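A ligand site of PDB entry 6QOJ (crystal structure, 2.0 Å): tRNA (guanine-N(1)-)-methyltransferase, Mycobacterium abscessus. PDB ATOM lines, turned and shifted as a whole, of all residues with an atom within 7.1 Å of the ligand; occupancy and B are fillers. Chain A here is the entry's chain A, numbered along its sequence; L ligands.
OH of Tyr 138 sits at hydrogen-bond distance from O of Ile 135, 3.1 Å away. O of Gly 136 sits at hydrogen-bond distance from OG of Ser 134 (2.8 Å). O of Val 133 sits at hydrogen-bond distance from N of Thr 86 (2.9 Å). O of Ser 134 is in hydrogen-bond range of N of Phe 92, 2.8 Å away. The backbone NH (N) of Gly 143 is in hydrogen-bond range of the backbone carbonyl oxygen (O) of Gly 111, at 2.9 Å. The backbone carbonyl oxygen of Val 84 is in hydrogen-bond range of the backbone NH of Val 133, at 3.2 Å. N of Tyr 113 lies within hydrogen-bond range of O of Asn 141.
The backbone NH (N) of Ile 135 sits at hydrogen-bond distance from an oxygen (O1) of the ligand, at 3.0 Å. The backbone carbonyl oxygen (O) of Gly 136 sits at hydrogen-bond distance from a nitrogen (N1) of the ligand, 3.1 Å away. The backbone NH of Leu 140 lies close to a nitrogen (N2) of the ligand.
Merely in contact with the ligand: Tyr 138 (3.0 Å), Thr 86 (3.2 Å), Ser 134 (3.2 Å), Gly 143 (3.4 Å), Gly 142 (3.4 Å), Pro 85 (3.4 Å), Pro 87 (3.7 Å), Val 133 (3.9 Å) and Tyr 113 (3.9 Å). Hydrophobic or aromatic side chains that line the ligand: Pro 85, Pro 87, Tyr 113, Ile 135 and Leu 140. Within 4 Å of the ligand: Pro 85, Thr 86, Pro 87, Tyr 113, Val 133, Ser 134, Ile 135, Gly 136, Tyr 138, Leu 140, Gly 142 and Gly 143. The nearest printed residue that does not touch the ligand is Gly 111 (4.03 Å).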
ATOM      1  N   VAL A  84       0.747  -0.820 -12.495  1.00  0.00           N
ATOM      2  CA  VAL A  84      -0.118   0.349 -12.536  1.00  0.00           C
ATOM      3  C   VAL A  84       0.466   1.367 -13.501  1.00  0.00           C
ATOM      4  O   VAL A  84       1.367   2.109 -13.139  1.00  0.00           O
ATOM      5  CB  VAL A  84      -0.261   1.009 -11.133  1.00  0.00           C
ATOM      6  CG1 VAL A  84      -1.268   2.152 -11.181  1.00  0.00           C
ATOM      7  CG2 VAL A  84      -0.642  -0.014 -10.088  1.00  0.00           C
ATOM      8  N   PRO A  85      -0.015   1.393 -14.737  1.00  0.00           N
ATOM      9  CA  PRO A  85       0.461   2.425 -15.640  1.00  0.00           C
ATOM     10  C   PRO A  85       0.128   3.828 -15.112  1.00  0.00           C
ATOM     11  O   PRO A  85      -0.952   4.036 -14.539  1.00  0.00           O
ATOM     12  CB  PRO A  85      -0.275   2.111 -16.942  1.00  0.00           C
ATOM     13  CG  PRO A  85      -0.432   0.592 -16.890  1.00  0.00           C
ATOM     14  CD  PRO A  85      -0.773   0.335 -15.436  1.00  0.00           C
ATOM     15  N   THR A  86       1.057   4.748 -15.277  1.00  0.00           N
ATOM     16  CA  THR A  86       0.955   6.100 -14.750  1.00  0.00           C
ATOM     17  C   THR A  86       2.009   6.982 -15.403  1.00  0.00           C
ATOM     18  O   THR A  86       3.167   6.583 -15.510  1.00  0.00           O
ATOM     19  CB  THR A  86       1.173   6.144 -13.229  1.00  0.00           C
ATOM     20  OG1 THR A  86       0.147   5.389 -12.572  1.00  0.00           O
ATOM     21  CG2 THR A  86       1.157   7.572 -12.714  1.00  0.00           C
ATOM     22  N   PRO A  87       1.614   8.185 -15.829  1.00  0.00           N
ATOM     23  CA  PRO A  87       2.590   9.168 -16.332  1.00  0.00           C
ATOM     24  C   PRO A  87       3.722   9.434 -15.326  1.00  0.00           C
ATOM     25  O   PRO A  87       4.815   9.840 -15.711  1.00  0.00           O
ATOM     26  CB  PRO A  87       1.744  10.429 -16.511  1.00  0.00           C
ATOM     27  CG  PRO A  87       0.498  10.186 -15.671  1.00  0.00           C
ATOM     28  CD  PRO A  87       0.251   8.729 -15.829  1.00  0.00           C
ATOM     29  N   ALA A  88       3.436   9.204 -14.047  1.00  0.00           N
ATOM     30  CA  ALA A  88       4.377   9.498 -12.979  1.00  0.00           C
ATOM     31  C   ALA A  88       5.189   8.277 -12.551  1.00  0.00           C
ATOM     32  O   ALA A  88       5.872   8.302 -11.533  1.00  0.00           O
ATOM     33  CB  ALA A  88       3.644  10.072 -11.791  1.00  0.00           C
ATOM     34  N   GLY A  89       5.136   7.208 -13.336  1.00  0.00           N
ATOM     35  CA  GLY A  89       5.832   5.986 -12.945  1.00  0.00           C
ATOM     36  C   GLY A  89       7.323   5.945 -13.242  1.00  0.00           C
ATOM     37  O   GLY A  89       7.856   6.818 -13.939  1.00  0.00           O
ATOM     38  N   PHE A  92       9.094   2.139 -17.972  1.00  0.00           N
ATOM     39  CA  PHE A  92       8.985   0.771 -18.443  1.00  0.00           C
ATOM     40  C   PHE A  92      10.026   0.578 -19.543  1.00  0.00           C
ATOM     41  O   PHE A  92       9.964   1.249 -20.577  1.00  0.00           O
ATOM     42  CB  PHE A  92       7.565   0.484 -18.975  1.00  0.00           C
ATOM     43  CG  PHE A  92       7.402  -0.884 -19.555  1.00  0.00           C
ATOM     44  CD1 PHE A  92       7.331  -1.988 -18.740  1.00  0.00           C
ATOM     45  CD2 PHE A  92       7.280  -1.052 -20.931  1.00  0.00           C
ATOM     46  CE1 PHE A  92       7.185  -3.272 -19.270  1.00  0.00           C
ATOM     47  CE2 PHE A  92       7.132  -2.336 -21.483  1.00  0.00           C
ATOM     48  CZ  PHE A  92       7.092  -3.445 -20.640  1.00  0.00           C
ATOM     49  N   ALA A 109      -3.662  -2.590 -13.510  1.00  0.00           N
ATOM     50  CA  ALA A 109      -4.714  -1.669 -13.108  1.00  0.00           C
ATOM     51  C   ALA A 109      -4.747  -0.452 -14.004  1.00  0.00           C
ATOM     52  O   ALA A 109      -3.855   0.405 -13.918  1.00  0.00           O
ATOM     53  CB  ALA A 109      -4.521  -1.244 -11.641  1.00  0.00           C
ATOM     54  N   CYS A 110      -5.768  -0.351 -14.863  1.00  0.00           N
ATOM     55  CA  CYS A 110      -5.891   0.779 -15.776  1.00  0.00           C
ATOM     56  C   CYS A 110      -6.689   1.939 -15.203  1.00  0.00           C
ATOM     57  O   CYS A 110      -7.874   1.790 -14.899  1.00  0.00           O
ATOM     58  CB  CYS A 110      -6.526   0.340 -17.100  1.00  0.00           C
ATOM     59  SG  CYS A 110      -5.628  -0.960 -17.936  1.00  0.00           S
ATOM     60  N   GLY A 111      -6.062   3.106 -15.081  1.00  0.00           N
ATOM     61  CA  GLY A 111      -6.749   4.266 -14.538  1.00  0.00           C
ATOM     62  C   GLY A 111      -6.554   5.513 -15.361  1.00  0.00           C
ATOM     63  O   GLY A 111      -5.659   5.573 -16.207  1.00  0.00           O
ATOM     64  N   ARG A 112      -7.382   6.521 -15.113  1.00  0.00           N
ATOM     65  CA  ARG A 112      -7.250   7.790 -15.820  1.00  0.00           C
ATOM     66  C   ARG A 112      -5.934   8.502 -15.500  1.00  0.00           C
ATOM     67  O   ARG A 112      -5.330   8.291 -14.442  1.00  0.00           O
ATOM     68  CB  ARG A 112      -8.421   8.709 -15.477  1.00  0.00           C
ATOM     69  CG  ARG A 112      -8.607   8.936 -14.009  1.00  0.00           C
ATOM     70  CD  ARG A 112      -9.909   9.659 -13.741  1.00  0.00           C
ATOM     71  NE  ARG A 112      -9.959  10.916 -14.479  1.00  0.00           N
ATOM     72  CZ  ARG A 112     -11.086  11.494 -14.879  1.00  0.00           C
ATOM     73  NH1 ARG A 112     -12.249  10.911 -14.617  1.00  0.00           N
ATOM     74  NH2 ARG A 112     -11.043  12.637 -15.553  1.00  0.00           N
ATOM     75  N   TYR A 113      -5.507   9.331 -16.443  1.00  0.00           N
ATOM     76  CA  TYR A 113      -4.287  10.103 -16.365  1.00  0.00           C
ATOM     77  C   TYR A 113      -4.070  10.814 -15.016  1.00  0.00           C
ATOM     78  O   TYR A 113      -2.962  10.804 -14.475  1.00  0.00           O
ATOM     79  CB  TYR A 113      -4.284  11.139 -17.504  1.00  0.00           C
ATOM     80  CG  TYR A 113      -3.071  12.020 -17.505  1.00  0.00           C
ATOM     81  CD1 TYR A 113      -1.854  11.553 -17.999  1.00  0.00           C
ATOM     82  CD2 TYR A 113      -3.126  13.319 -17.011  1.00  0.00           C
ATOM     83  CE1 TYR A 113      -0.728  12.358 -18.009  1.00  0.00           C
ATOM     84  CE2 TYR A 113      -1.995  14.124 -17.012  1.00  0.00           C
ATOM     85  CZ  TYR A 113      -0.797  13.634 -17.504  1.00  0.00           C
ATOM     86  OH  TYR A 113       0.331  14.429 -17.514  1.00  0.00           O
ATOM     87  N   GLU A 114      -5.136  11.420 -14.487  1.00  0.00           N
ATOM     88  CA  GLU A 114      -5.079  12.153 -13.221  1.00  0.00           C
ATOM     89  C   GLU A 114      -4.721  11.241 -12.076  1.00  0.00           C
ATOM     90  O   GLU A 114      -4.277  11.692 -11.026  1.00  0.00           O
ATOM     91  CB  GLU A 114      -6.408  12.850 -12.946  1.00  0.00           C
ATOM     92  CG  GLU A 114      -6.739  13.943 -13.920  1.00  0.00           C
ATOM     93  CD  GLU A 114      -7.259  13.413 -15.253  1.00  0.00           C
ATOM     94  OE1 GLU A 114      -7.466  12.186 -15.381  1.00  0.00           O
ATOM     95  OE2 GLU A 114      -7.442  14.227 -16.175  1.00  0.00           O
ATOM     96  N   GLY A 115      -4.913   9.945 -12.274  1.00  0.00           N
ATOM     97  CA  GLY A 115      -4.438   8.948 -11.349  1.00  0.00           C
ATOM     98  C   GLY A 115      -5.523   8.255 -10.560  1.00  0.00           C
ATOM     99  O   GLY A 115      -6.669   8.696 -10.501  1.00  0.00           O
ATOM    100  N   VAL A 133       4.545   2.362 -13.435  1.00  0.00           N
ATOM    101  CA  VAL A 133       5.426   2.556 -14.580  1.00  0.00           C
ATOM    102  C   VAL A 133       4.822   3.437 -15.671  1.00  0.00           C
ATOM    103  O   VAL A 133       3.606   3.465 -15.859  1.00  0.00           O
ATOM    104  CB  VAL A 133       5.846   1.207 -15.224  1.00  0.00           C
ATOM    105  CG1 VAL A 133       6.635   0.326 -14.217  1.00  0.00           C
ATOM    106  CG2 VAL A 133       4.642   0.449 -15.779  1.00  0.00           C
ATOM    107  N   SER A 134       5.694   4.123 -16.404  1.00  0.00           N
ATOM    108  CA  SER A 134       5.280   4.893 -17.582  1.00  0.00           C
ATOM    109  C   SER A 134       5.906   4.320 -18.847  1.00  0.00           C
ATOM    110  O   SER A 134       7.065   3.933 -18.851  1.00  0.00           O
ATOM    111  CB  SER A 134       5.673   6.375 -17.431  1.00  0.00           C
ATOM    112  OG  SER A 134       5.483   7.061 -18.671  1.00  0.00           O
ATOM    113  N   ILE A 135       5.129   4.287 -19.926  1.00  0.00           N
ATOM    114  CA  ILE A 135       5.636   3.795 -21.190  1.00  0.00           C
ATOM    115  C   ILE A 135       6.160   4.936 -22.064  1.00  0.00           C
ATOM    116  O   ILE A 135       6.688   4.714 -23.163  1.00  0.00           O
ATOM    117  CB  ILE A 135       4.562   3.036 -21.961  1.00  0.00           C
ATOM    118  CG1 ILE A 135       3.385   3.951 -22.313  1.00  0.00           C
ATOM    119  CG2 ILE A 135       4.106   1.803 -21.173  1.00  0.00           C
ATOM    120  CD1 ILE A 135       2.611   3.470 -23.526  1.00  0.00           C
ATOM    121  N   GLY A 136       6.028   6.161 -21.562  1.00  0.00           N
ATOM    122  CA  GLY A 136       6.461   7.319 -22.328  1.00  0.00           C
ATOM    123  C   GLY A 136       5.901   8.602 -21.757  1.00  0.00           C
ATOM    124  O   GLY A 136       4.951   8.592 -20.990  1.00  0.00           O
ATOM    125  N   ASP A 137       6.505   9.725 -22.153  1.00  0.00           N
ATOM    126  CA  ASP A 137       6.161  11.015 -21.593  1.00  0.00           C
ATOM    127  C   ASP A 137       5.163  11.811 -22.443  1.00  0.00           C
ATOM    128  O   ASP A 137       4.839  12.959 -22.123  1.00  0.00           O
ATOM    129  CB  ASP A 137       7.436  11.820 -21.376  1.00  0.00           C
ATOM    130  CG  ASP A 137       8.253  11.293 -20.207  1.00  0.00           C
ATOM    131  OD1 ASP A 137       7.688  10.559 -19.369  1.00  0.00           O
ATOM    132  OD2 ASP A 137       9.463  11.626 -20.128  1.00  0.00           O
ATOM    133  N   TYR A 138       4.664  11.198 -23.510  1.00  0.00           N
ATOM    134  CA  TYR A 138       3.464  11.719 -24.163  1.00  0.00           C
ATOM    135  C   TYR A 138       2.314  11.444 -23.212  1.00  0.00           C
ATOM    136  O   TYR A 138       2.452  10.673 -22.257  1.00  0.00           O
ATOM    137  CB  TYR A 138       3.238  11.056 -25.513  1.00  0.00           C
ATOM    138  CG  TYR A 138       3.624   9.601 -25.483  1.00  0.00           C
ATOM    139  CD1 TYR A 138       2.783   8.663 -24.902  1.00  0.00           C
ATOM    140  CD2 TYR A 138       4.843   9.164 -26.005  1.00  0.00           C
ATOM    141  CE1 TYR A 138       3.113   7.361 -24.845  1.00  0.00           C
ATOM    142  CE2 TYR A 138       5.177   7.822 -25.970  1.00  0.00           C
ATOM    143  CZ  TYR A 138       4.316   6.932 -25.371  1.00  0.00           C
ATOM    144  OH  TYR A 138       4.637   5.608 -25.296  1.00  0.00           O
ATOM    145  N   VAL A 139       1.162  12.041 -23.471  1.00  0.00           N
ATOM    146  CA  VAL A 139       0.083  11.941 -22.512  1.00  0.00           C
ATOM    147  C   VAL A 139      -1.079  11.171 -23.079  1.00  0.00           C
ATOM    148  O   VAL A 139      -1.675  11.577 -24.072  1.00  0.00           O
ATOM    149  CB  VAL A 139      -0.416  13.334 -22.084  1.00  0.00           C
ATOM    150  CG1 VAL A 139      -1.677  13.201 -21.259  1.00  0.00           C
ATOM    151  CG2 VAL A 139       0.682  14.067 -21.300  1.00  0.00           C
ATOM    152  N   LEU A 140      -1.407  10.059 -22.439  1.00  0.00           N
ATOM    153  CA  LEU A 140      -2.590   9.279 -22.771  1.00  0.00           C
ATOM    154  C   LEU A 140      -3.670   9.626 -21.772  1.00  0.00           C
ATOM    155  O   LEU A 140      -3.379  10.022 -20.639  1.00  0.00           O
ATOM    156  CB  LEU A 140      -2.292   7.789 -22.721  1.00  0.00           C
ATOM    157  CG  LEU A 140      -1.089   7.313 -23.532  1.00  0.00           C
ATOM    158  CD1 LEU A 140      -0.788   5.880 -23.187  1.00  0.00           C
ATOM    159  CD2 LEU A 140      -1.344   7.476 -25.021  1.00  0.00           C
ATOM    160  N   ASN A 141      -4.929   9.461 -22.180  1.00  0.00           N
ATOM    161  CA  ASN A 141      -6.034   9.792 -21.304  1.00  0.00           C
ATOM    162  C   ASN A 141      -6.287   8.763 -20.206  1.00  0.00           C
ATOM    163  O   ASN A 141      -6.839   9.102 -19.154  1.00  0.00           O
ATOM    164  CB  ASN A 141      -7.314  10.002 -22.094  1.00  0.00           C
ATOM    165  CG  ASN A 141      -8.207  11.036 -21.439  1.00  0.00           C
ATOM    166  OD1 ASN A 141      -7.960  12.234 -21.564  1.00  0.00           O
ATOM    167  ND2 ASN A 141      -9.235  10.575 -20.746  1.00  0.00           N
ATOM    168  N   GLY A 142      -5.904   7.515 -20.455  1.00  0.00           N
ATOM    169  CA  GLY A 142      -6.010   6.490 -19.444  1.00  0.00           C
ATOM    170  C   GLY A 142      -4.921   5.447 -19.642  1.00  0.00           C
ATOM    171  O   GLY A 142      -4.173   5.509 -20.612  1.00  0.00           O
ATOM    172  N   GLY A 143      -4.837   4.493 -18.726  1.00  0.00           N
ATOM    173  CA  GLY A 143      -3.800   3.475 -18.769  1.00  0.00           C
ATOM    174  C   GLY A 143      -4.039   2.360 -19.777  1.00  0.00           C
ATOM    175  O   GLY A 143      -3.191   1.469 -19.923  1.00  0.00           O
ATOM    176  N   GLU A 144      -5.172   2.394 -20.469  1.00  0.00           N
ATOM    177  CA  GLU A 144      -5.565   1.285 -21.341  1.00  0.00           C
ATOM    178  C   GLU A 144      -4.557   0.994 -22.444  1.00  0.00           C
ATOM    179  O   GLU A 144      -4.078  -0.134 -22.601  1.00  0.00           O
ATOM    180  CB  GLU A 144      -6.949   1.540 -21.959  1.00  0.00           C
ATOM    181  CG  GLU A 144      -8.140   1.309 -21.024  1.00  0.00           C
ATOM    182  CD  GLU A 144      -8.215   2.332 -19.879  1.00  0.00           C
ATOM    183  OE1 GLU A 144      -7.622   3.427 -20.008  1.00  0.00           O
ATOM    184  OE2 GLU A 144      -8.867   2.023 -18.855  1.00  0.00           O
ATOM    185  N   ALA A 146      -1.529   1.903 -22.638  1.00  0.00           N
ATOM    186  CA  ALA A 146      -0.252   1.537 -22.049  1.00  0.00           C
ATOM    187  C   ALA A 146      -0.270   0.059 -21.640  1.00  0.00           C
ATOM    188  O   ALA A 146       0.750  -0.619 -21.737  1.00  0.00           O
ATOM    189  CB  ALA A 146       0.077   2.427 -20.857  1.00  0.00           C
ATOM    190  N   ALA A 147      -1.422  -0.428 -21.198  1.00  0.00           N
ATOM    191  CA  ALA A 147      -1.564  -1.828 -20.854  1.00  0.00           C
ATOM    192  C   ALA A 147      -1.383  -2.712 -22.100  1.00  0.00           C
ATOM    193  O   ALA A 147      -0.729  -3.764 -22.043  1.00  0.00           O
ATOM    194  CB  ALA A 147      -2.920  -2.073 -20.216  1.00  0.00           C
ATOM    195  N   ILE A 150       2.395  -2.758 -22.852  1.00  0.00           N
ATOM    196  CA  ILE A 150       3.075  -3.618 -21.901  1.00  0.00           C
ATOM    197  C   ILE A 150       2.844  -5.095 -22.194  1.00  0.00           C
ATOM    198  O   ILE A 150       3.785  -5.915 -22.147  1.00  0.00           O
ATOM    199  CB  ILE A 150       2.608  -3.257 -20.470  1.00  0.00           C
ATOM    200  CG1 ILE A 150       3.270  -1.947 -20.036  1.00  0.00           C
ATOM    201  CG2 ILE A 150       3.007  -4.318 -19.493  1.00  0.00           C
ATOM    202  CD1 ILE A 150       2.610  -1.278 -18.821  1.00  0.00           C
HETATM  203  C1  LIG L   1      -0.219   5.532 -18.072  1.00  0.00           C
HETATM  204  O1  LIG L   1       2.450   5.227 -19.087  1.00  0.00           O
HETATM  205  C2  LIG L   1       1.697   6.348 -19.444  1.00  0.00           C
HETATM  206  N1  LIG L   1       2.211   7.286 -20.253  1.00  0.00           N
HETATM  207  C3  LIG L   1       1.486   8.361 -20.633  1.00  0.00           C
HETATM  208  N2  LIG L   1       0.224   8.515 -20.181  1.00  0.00           N
HETATM  209  C4  LIG L   1      -0.347   7.589 -19.327  1.00  0.00           C
HETATM  210  C5  LIG L   1      -1.687   7.760 -18.842  1.00  0.00           C
HETATM  211  C6  LIG L   1      -2.267   6.832 -17.984  1.00  0.00           C
HETATM  212  C7  LIG L   1      -1.520   5.710 -17.599  1.00  0.00           C
HETATM  213  C8  LIG L   1       0.366   6.501 -18.950  1.00  0.00           C
